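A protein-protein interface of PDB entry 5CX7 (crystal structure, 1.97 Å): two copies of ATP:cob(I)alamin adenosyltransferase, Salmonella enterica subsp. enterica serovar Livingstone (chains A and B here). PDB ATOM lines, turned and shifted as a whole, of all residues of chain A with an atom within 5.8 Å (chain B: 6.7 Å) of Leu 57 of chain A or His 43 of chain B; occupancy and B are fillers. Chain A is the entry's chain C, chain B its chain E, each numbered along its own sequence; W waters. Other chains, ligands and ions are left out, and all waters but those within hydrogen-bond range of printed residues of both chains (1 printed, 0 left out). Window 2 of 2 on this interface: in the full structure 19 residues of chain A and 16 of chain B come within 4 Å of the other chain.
N of Leu 57 of chain A sits at hydrogen-bond distance from O of Ala 72 of chain B (3.3 Å). N of Val 58 of chain A sits at hydrogen-bond distance from O of Ala 72 of chain B.
The side-chain hydroxyl (OG) of Ser 59 of chain A lies close to the backbone carbonyl oxygen (O) of Leu 56 of chain A, at 3.5 Å. N of His 43 of chain B sits at hydrogen-bond distance from OD1 of Asp 41 of chain B, at 2.9 Å.
Leu 56 of chain A touches Ala 72 of chain B. Leu 56 of chain A touches Met 73 of chain B. Leu 56 of chain A touches Lys 74 of chain B (CD2 to CD, 3.7 Å). Leu 57 of chain A touches His 43 of chain B (CD2 to O, 3.6 Å). Trp 68 of chain B touches Leu 57 of chain A. Val 58 of chain A touches Met 73 of chain B (CG1 to CG, 3.7 Å). CD1 of Leu 97 of chain B touches CG1 of Val 58 of chain A (3.6 Å). Glu 61 of chain A touches Leu 97 of chain B (CD to CD2, 3.7 Å).
Leu 57 of chain A touches three residues of chain B. His 43 of chain B touches one residue of chain A. Printed residues of chain B within 4 Å of Val 58 of chain A: Ala 72, Met 73 and Leu 97. Printed residues of chain A within 4 Å of Lys 74 of chain B: Leu 56 (3.7 Å). Printed residues of chain B within 4 Å of Glu 61 of chain A: Leu 97 (3.7 Å). Printed residues of chain A within 4 Å of Ala 72 of chain B: Leu 56, Leu 57 and Val 58. Val 71 of chain B touches none of the printed residues of chain A. The nearest residue of chain B that does not touch Leu 57 of chain A is Gly 44 of chain B (4.7 Å). The nearest printed residue of chain A that does not touch His 43 of chain B is Arg 51 of chain A (7.5 Å).
Of the 15 printed residues of chain B, 6 touch a printed residue of chain A. Hydrophobic or aromatic side chains of chain B that line the printed part of chain A: Trp 68, Ala 72, Met 73 and Leu 97. Of the 8 printed residues of chain A, 4 touch a printed residue of chain B. Hydrophobic or aromatic side chains of chain A within 4 Å of the printed part of chain B: Leu 56, Leu 57 and Val 58. Among the printed residues, 10 pairs touch across the chains. Among the printed residues, no Asp or Glu carboxylate lies within 4 Å of a Lys or Arg side-chain nitrogen of the other chain.
No position is printed for both chains.
Water W1 lies within hydrogen-bond range of O of Val 71 of chain B, N of Leu 57 of chain A and O of Ala 72 of chain B.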
ATOM      1  N   ARG A  51      36.560  -8.197  -1.628  1.00  0.00           N
ATOM      2  CA  ARG A  51      35.915  -9.399  -2.073  1.00  0.00           C
ATOM      3  C   ARG A  51      36.300  -9.728  -3.481  1.00  0.00           C
ATOM      4  O   ARG A  51      36.010  -8.952  -4.392  1.00  0.00           O
ATOM      5  CB  ARG A  51      34.392  -9.253  -1.996  1.00  0.00           C
ATOM      6  CG  ARG A  51      33.601 -10.439  -2.542  1.00  0.00           C
ATOM      7  CD  ARG A  51      32.083 -10.302  -2.281  1.00  0.00           C
ATOM      8  NE  ARG A  51      31.401 -11.538  -2.706  1.00  0.00           N
ATOM      9  CZ  ARG A  51      30.962 -11.807  -3.938  1.00  0.00           C
ATOM     10  NH1 ARG A  51      31.020 -10.924  -4.941  1.00  0.00           N
ATOM     11  NH2 ARG A  51      30.441 -13.015  -4.185  1.00  0.00           N
ATOM     12  N   ALA A  55      33.202 -15.107  -4.551  1.00  0.00           N
ATOM     13  CA  ALA A  55      33.462 -15.619  -3.216  1.00  0.00           C
ATOM     14  C   ALA A  55      32.126 -16.029  -2.567  1.00  0.00           C
ATOM     15  O   ALA A  55      31.084 -15.384  -2.779  1.00  0.00           O
ATOM     16  CB  ALA A  55      34.173 -14.580  -2.326  1.00  0.00           C
ATOM     17  N   LEU A  56      32.140 -17.076  -1.787  1.00  0.00           N
ATOM     18  CA  LEU A  56      30.949 -17.506  -1.080  1.00  0.00           C
ATOM     19  C   LEU A  56      30.331 -16.345  -0.339  1.00  0.00           C
ATOM     20  O   LEU A  56      31.051 -15.598   0.303  1.00  0.00           O
ATOM     21  CB  LEU A  56      31.276 -18.590  -0.010  1.00  0.00           C
ATOM     22  CG  LEU A  56      31.818 -19.951  -0.416  1.00  0.00           C
ATOM     23  CD1 LEU A  56      32.109 -20.790   0.789  1.00  0.00           C
ATOM     24  CD2 LEU A  56      30.828 -20.648  -1.344  1.00  0.00           C
ATOM     25  N   LEU A  57      29.016 -16.175  -0.452  1.00  0.00           N
ATOM     26  CA  LEU A  57      28.358 -15.095   0.211  1.00  0.00           C
ATOM     27  C   LEU A  57      28.637 -15.054   1.768  1.00  0.00           C
ATOM     28  O   LEU A  57      28.832 -13.973   2.289  1.00  0.00           O
ATOM     29  CB  LEU A  57      26.819 -15.084  -0.057  1.00  0.00           C
ATOM     30  CG  LEU A  57      25.903 -14.044   0.374  1.00  0.00           C
ATOM     31  CD1 LEU A  57      26.581 -12.747   0.191  1.00  0.00           C
ATOM     32  CD2 LEU A  57      24.514 -14.073  -0.328  1.00  0.00           C
ATOM     33  N   VAL A  58      28.682 -16.221   2.434  1.00  0.00           N
ATOM     34  CA  VAL A  58      29.008 -16.288   3.865  1.00  0.00           C
ATOM     35  C   VAL A  58      30.355 -15.639   4.231  1.00  0.00           C
ATOM     36  O   VAL A  58      30.490 -15.131   5.301  1.00  0.00           O
ATOM     37  CB  VAL A  58      28.952 -17.699   4.454  1.00  0.00           C
ATOM     38  CG1 VAL A  58      27.543 -18.263   4.370  1.00  0.00           C
ATOM     39  CG2 VAL A  58      29.971 -18.646   3.835  1.00  0.00           C
ATOM     40  N   SER A  59      31.294 -15.638   3.272  1.00  0.00           N
ATOM     41  CA  SER A  59      32.590 -15.108   3.511  1.00  0.00           C
ATOM     42  C   SER A  59      32.597 -13.593   3.813  1.00  0.00           C
ATOM     43  O   SER A  59      33.517 -13.127   4.443  1.00  0.00           O
ATOM     44  CB  SER A  59      33.501 -15.497   2.357  1.00  0.00           C
ATOM     45  OG  SER A  59      33.579 -16.936   2.317  1.00  0.00           O
ATOM     46  N   SER A  60      31.624 -12.858   3.272  1.00  0.00           N
ATOM     47  CA  SER A  60      31.431 -11.461   3.520  1.00  0.00           C
ATOM     48  C   SER A  60      31.216 -11.153   5.035  1.00  0.00           C
ATOM     49  O   SER A  60      31.611 -10.112   5.476  1.00  0.00           O
ATOM     50  CB  SER A  60      30.284 -10.867   2.707  1.00  0.00           C
ATOM     51  OG  SER A  60      30.638 -10.906   1.318  1.00  0.00           O
ATOM     52  N   GLU A  61      30.640 -12.102   5.761  1.00  0.00           N
ATOM     53  CA  GLU A  61      30.428 -11.977   7.188  1.00  0.00           C
ATOM     54  C   GLU A  61      31.571 -12.697   7.937  1.00  0.00           C
ATOM     55  O   GLU A  61      32.147 -12.139   8.881  1.00  0.00           O
ATOM     56  CB  GLU A  61      29.066 -12.608   7.537  1.00  0.00           C
ATOM     57  CG  GLU A  61      28.738 -12.524   9.005  1.00  0.00           C
ATOM     58  CD  GLU A  61      27.259 -12.733   9.306  1.00  0.00           C
ATOM     59  OE1 GLU A  61      26.443 -12.736   8.353  1.00  0.00           O
ATOM     60  OE2 GLU A  61      26.918 -12.826  10.505  1.00  0.00           O
ATOM     61  N   VAL B  40      15.225 -18.755  -3.640  1.00  0.00           N
ATOM     62  CA  VAL B  40      16.078 -17.579  -3.746  1.00  0.00           C
ATOM     63  C   VAL B  40      16.858 -17.624  -5.081  1.00  0.00           C
ATOM     64  O   VAL B  40      16.998 -18.669  -5.697  1.00  0.00           O
ATOM     65  CB  VAL B  40      17.049 -17.417  -2.554  1.00  0.00           C
ATOM     66  CG1 VAL B  40      16.312 -17.373  -1.237  1.00  0.00           C
ATOM     67  CG2 VAL B  40      18.091 -18.508  -2.555  1.00  0.00           C
ATOM     68  N   ASP B  41      17.236 -16.461  -5.568  1.00  0.00           N
ATOM     69  CA  ASP B  41      18.041 -16.365  -6.763  1.00  0.00           C
ATOM     70  C   ASP B  41      19.511 -16.596  -6.449  1.00  0.00           C
ATOM     71  O   ASP B  41      19.894 -16.883  -5.308  1.00  0.00           O
ATOM     72  CB  ASP B  41      17.751 -15.051  -7.537  1.00  0.00           C
ATOM     73  CG  ASP B  41      18.286 -13.801  -6.841  1.00  0.00           C
ATOM     74  OD1 ASP B  41      19.078 -13.875  -5.888  1.00  0.00           O
ATOM     75  OD2 ASP B  41      17.835 -12.734  -7.296  1.00  0.00           O
ATOM     76  N   ALA B  42      20.357 -16.502  -7.469  1.00  0.00           N
ATOM     77  CA  ALA B  42      21.791 -16.744  -7.283  1.00  0.00           C
ATOM     78  C   ALA B  42      22.473 -15.779  -6.340  1.00  0.00           C
ATOM     79  O   ALA B  42      23.569 -16.071  -5.881  1.00  0.00           O
ATOM     80  CB  ALA B  42      22.520 -16.704  -8.642  1.00  0.00           C
ATOM     81  N   HIS B  43      21.866 -14.641  -6.053  1.00  0.00           N
ATOM     82  CA  HIS B  43      22.438 -13.675  -5.089  1.00  0.00           C
ATOM     83  C   HIS B  43      21.818 -13.824  -3.710  1.00  0.00           C
ATOM     84  O   HIS B  43      22.107 -13.068  -2.809  1.00  0.00           O
ATOM     85  CB  HIS B  43      22.226 -12.265  -5.673  1.00  0.00           C
ATOM     86  CG  HIS B  43      22.519 -12.222  -7.136  1.00  0.00           C
ATOM     87  ND1 HIS B  43      23.783 -12.451  -7.639  1.00  0.00           N
ATOM     88  CD2 HIS B  43      21.693 -12.142  -8.207  1.00  0.00           C
ATOM     89  CE1 HIS B  43      23.730 -12.460  -8.956  1.00  0.00           C
ATOM     90  NE2 HIS B  43      22.475 -12.277  -9.326  1.00  0.00           N
ATOM     91  N   GLY B  44      20.973 -14.827  -3.522  1.00  0.00           N
ATOM     92  CA  GLY B  44      20.300 -15.047  -2.232  1.00  0.00           C
ATOM     93  C   GLY B  44      19.062 -14.205  -1.955  1.00  0.00           C
ATOM     94  O   GLY B  44      18.529 -14.271  -0.870  1.00  0.00           O
ATOM     95  N   THR B  45      18.567 -13.475  -2.946  1.00  0.00           N
ATOM     96  CA  THR B  45      17.371 -12.713  -2.769  1.00  0.00           C
ATOM     97  C   THR B  45      16.166 -13.613  -2.823  1.00  0.00           C
ATOM     98  O   THR B  45      15.947 -14.356  -3.831  1.00  0.00           O
ATOM     99  CB  THR B  45      17.247 -11.606  -3.832  1.00  0.00           C
ATOM    100  OG1 THR B  45      18.426 -10.797  -3.753  1.00  0.00           O
ATOM    101  CG2 THR B  45      16.009 -10.703  -3.630  1.00  0.00           C
ATOM    102  N   TRP B  68      18.562 -19.825   1.194  1.00  0.00           N
ATOM    103  CA  TRP B  68      19.680 -18.892   1.225  1.00  0.00           C
ATOM    104  C   TRP B  68      21.031 -19.577   1.511  1.00  0.00           C
ATOM    105  O   TRP B  68      22.031 -19.267   0.838  1.00  0.00           O
ATOM    106  CB  TRP B  68      19.445 -17.817   2.308  1.00  0.00           C
ATOM    107  CG  TRP B  68      20.486 -16.766   2.266  1.00  0.00           C
ATOM    108  CD1 TRP B  68      20.473 -15.648   1.535  1.00  0.00           C
ATOM    109  CD2 TRP B  68      21.651 -16.695   3.072  1.00  0.00           C
ATOM    110  NE1 TRP B  68      21.591 -14.864   1.786  1.00  0.00           N
ATOM    111  CE2 TRP B  68      22.332 -15.471   2.731  1.00  0.00           C
ATOM    112  CE3 TRP B  68      22.203 -17.513   4.048  1.00  0.00           C
ATOM    113  CZ2 TRP B  68      23.493 -15.064   3.351  1.00  0.00           C
ATOM    114  CZ3 TRP B  68      23.448 -17.143   4.593  1.00  0.00           C
ATOM    115  CH2 TRP B  68      24.031 -15.916   4.280  1.00  0.00           C
ATOM    116  N   VAL B  71      22.659 -21.240  -1.548  1.00  0.00           N
ATOM    117  CA  VAL B  71      23.368 -20.319  -2.416  1.00  0.00           C
ATOM    118  C   VAL B  71      24.626 -19.737  -1.733  1.00  0.00           C
ATOM    119  O   VAL B  71      25.728 -19.671  -2.365  1.00  0.00           O
ATOM    120  CB  VAL B  71      22.408 -19.212  -2.908  1.00  0.00           C
ATOM    121  CG1 VAL B  71      23.061 -17.918  -3.454  1.00  0.00           C
ATOM    122  CG2 VAL B  71      21.400 -19.728  -3.935  1.00  0.00           C
ATOM    123  N   ALA B  72      24.473 -19.353  -0.469  1.00  0.00           N
ATOM    124  CA  ALA B  72      25.552 -18.673   0.290  1.00  0.00           C
ATOM    125  C   ALA B  72      26.761 -19.549   0.567  1.00  0.00           C
ATOM    126  O   ALA B  72      27.862 -19.052   0.757  1.00  0.00           O
ATOM    127  CB  ALA B  72      24.978 -18.136   1.623  1.00  0.00           C
ATOM    128  N   MET B  73      26.553 -20.879   0.620  1.00  0.00           N
ATOM    129  CA  MET B  73      27.574 -21.870   0.747  1.00  0.00           C
ATOM    130  C   MET B  73      27.756 -22.812  -0.488  1.00  0.00           C
ATOM    131  O   MET B  73      28.588 -23.714  -0.401  1.00  0.00           O
ATOM    132  CB  MET B  73      27.314 -22.705   1.970  1.00  0.00           C
ATOM    133  CG  MET B  73      27.216 -21.735   3.142  1.00  0.00           C
ATOM    134  SD  MET B  73      27.778 -22.284   4.670  1.00  0.00           S
ATOM    135  CE  MET B  73      29.477 -22.670   4.324  1.00  0.00           C
ATOM    136  N   LYS B  74      27.014 -22.565  -1.546  1.00  0.00           N
ATOM    137  CA  LYS B  74      27.073 -23.376  -2.779  1.00  0.00           C
ATOM    138  C   LYS B  74      26.981 -24.856  -2.491  1.00  0.00           C
ATOM    139  O   LYS B  74      27.780 -25.662  -2.970  1.00  0.00           O
ATOM    140  CB  LYS B  74      28.335 -23.051  -3.595  1.00  0.00           C
ATOM    141  CG  LYS B  74      28.379 -21.657  -4.062  1.00  0.00           C
ATOM    142  CD  LYS B  74      29.710 -21.383  -4.829  1.00  0.00           C
ATOM    143  CE  LYS B  74      29.866 -19.940  -5.163  1.00  0.00           C
ATOM    144  NZ  LYS B  74      31.213 -19.657  -5.785  1.00  0.00           N
ATOM    145  N   LEU B  97      27.059 -17.131  11.980  1.00  0.00           N
ATOM    146  CA  LEU B  97      26.326 -16.446  10.998  1.00  0.00           C
ATOM    147  C   LEU B  97      24.936 -16.039  11.557  1.00  0.00           C
ATOM    148  O   LEU B  97      24.048 -15.720  10.761  1.00  0.00           O
ATOM    149  CB  LEU B  97      26.221 -17.341   9.755  1.00  0.00           C
ATOM    150  CG  LEU B  97      27.581 -17.532   9.074  1.00  0.00           C
ATOM    151  CD1 LEU B  97      27.443 -18.555   7.989  1.00  0.00           C
ATOM    152  CD2 LEU B  97      28.082 -16.208   8.502  1.00  0.00           C
ATOM    153  N   LEU B 116      25.597 -21.207 -11.026  1.00  0.00           N
ATOM    154  CA  LEU B 116      24.669 -21.215  -9.907  1.00  0.00           C
ATOM    155  C   LEU B 116      23.530 -20.270 -10.220  1.00  0.00           C
ATOM    156  O   LEU B 116      23.709 -19.076 -10.470  1.00  0.00           O
ATOM    157  CB  LEU B 116      25.364 -20.745  -8.632  1.00  0.00           C
ATOM    158  CG  LEU B 116      24.467 -20.654  -7.371  1.00  0.00           C
ATOM    159  CD1 LEU B 116      24.056 -22.041  -6.955  1.00  0.00           C
ATOM    160  CD2 LEU B 116      25.223 -19.948  -6.256  1.00  0.00           C
ATOM    161  N   ILE B 117      22.293 -20.767 -10.159  1.00  0.00           N
ATOM    162  CA  ILE B 117      21.142 -19.908 -10.510  1.00  0.00           C
ATOM    163  C   ILE B 117      20.159 -19.636  -9.359  1.00  0.00           C
ATOM    164  O   ILE B 117      19.230 -18.845  -9.541  1.00  0.00           O
ATOM    165  CB  ILE B 117      20.352 -20.450 -11.768  1.00  0.00           C
ATOM    166  CG1 ILE B 117      19.774 -21.859 -11.582  1.00  0.00           C
ATOM    167  CG2 ILE B 117      21.288 -20.470 -13.001  1.00  0.00           C
ATOM    168  CD1 ILE B 117      18.873 -22.318 -12.763  1.00  0.00           C
ATOM    169  N   GLY B 118      20.293 -20.373  -8.273  1.00  0.00           N
ATOM    170  CA  GLY B 118      19.367 -20.195  -7.177  1.00  0.00           C
ATOM    171  C   GLY B 118      19.493 -21.283  -6.159  1.00  0.00           C
ATOM    172  O   GLY B 118      20.380 -22.112  -6.202  1.00  0.00           O
HETATM  173  O   HOH W   1      27.827 -17.901  -2.529  1.00  0.00           O
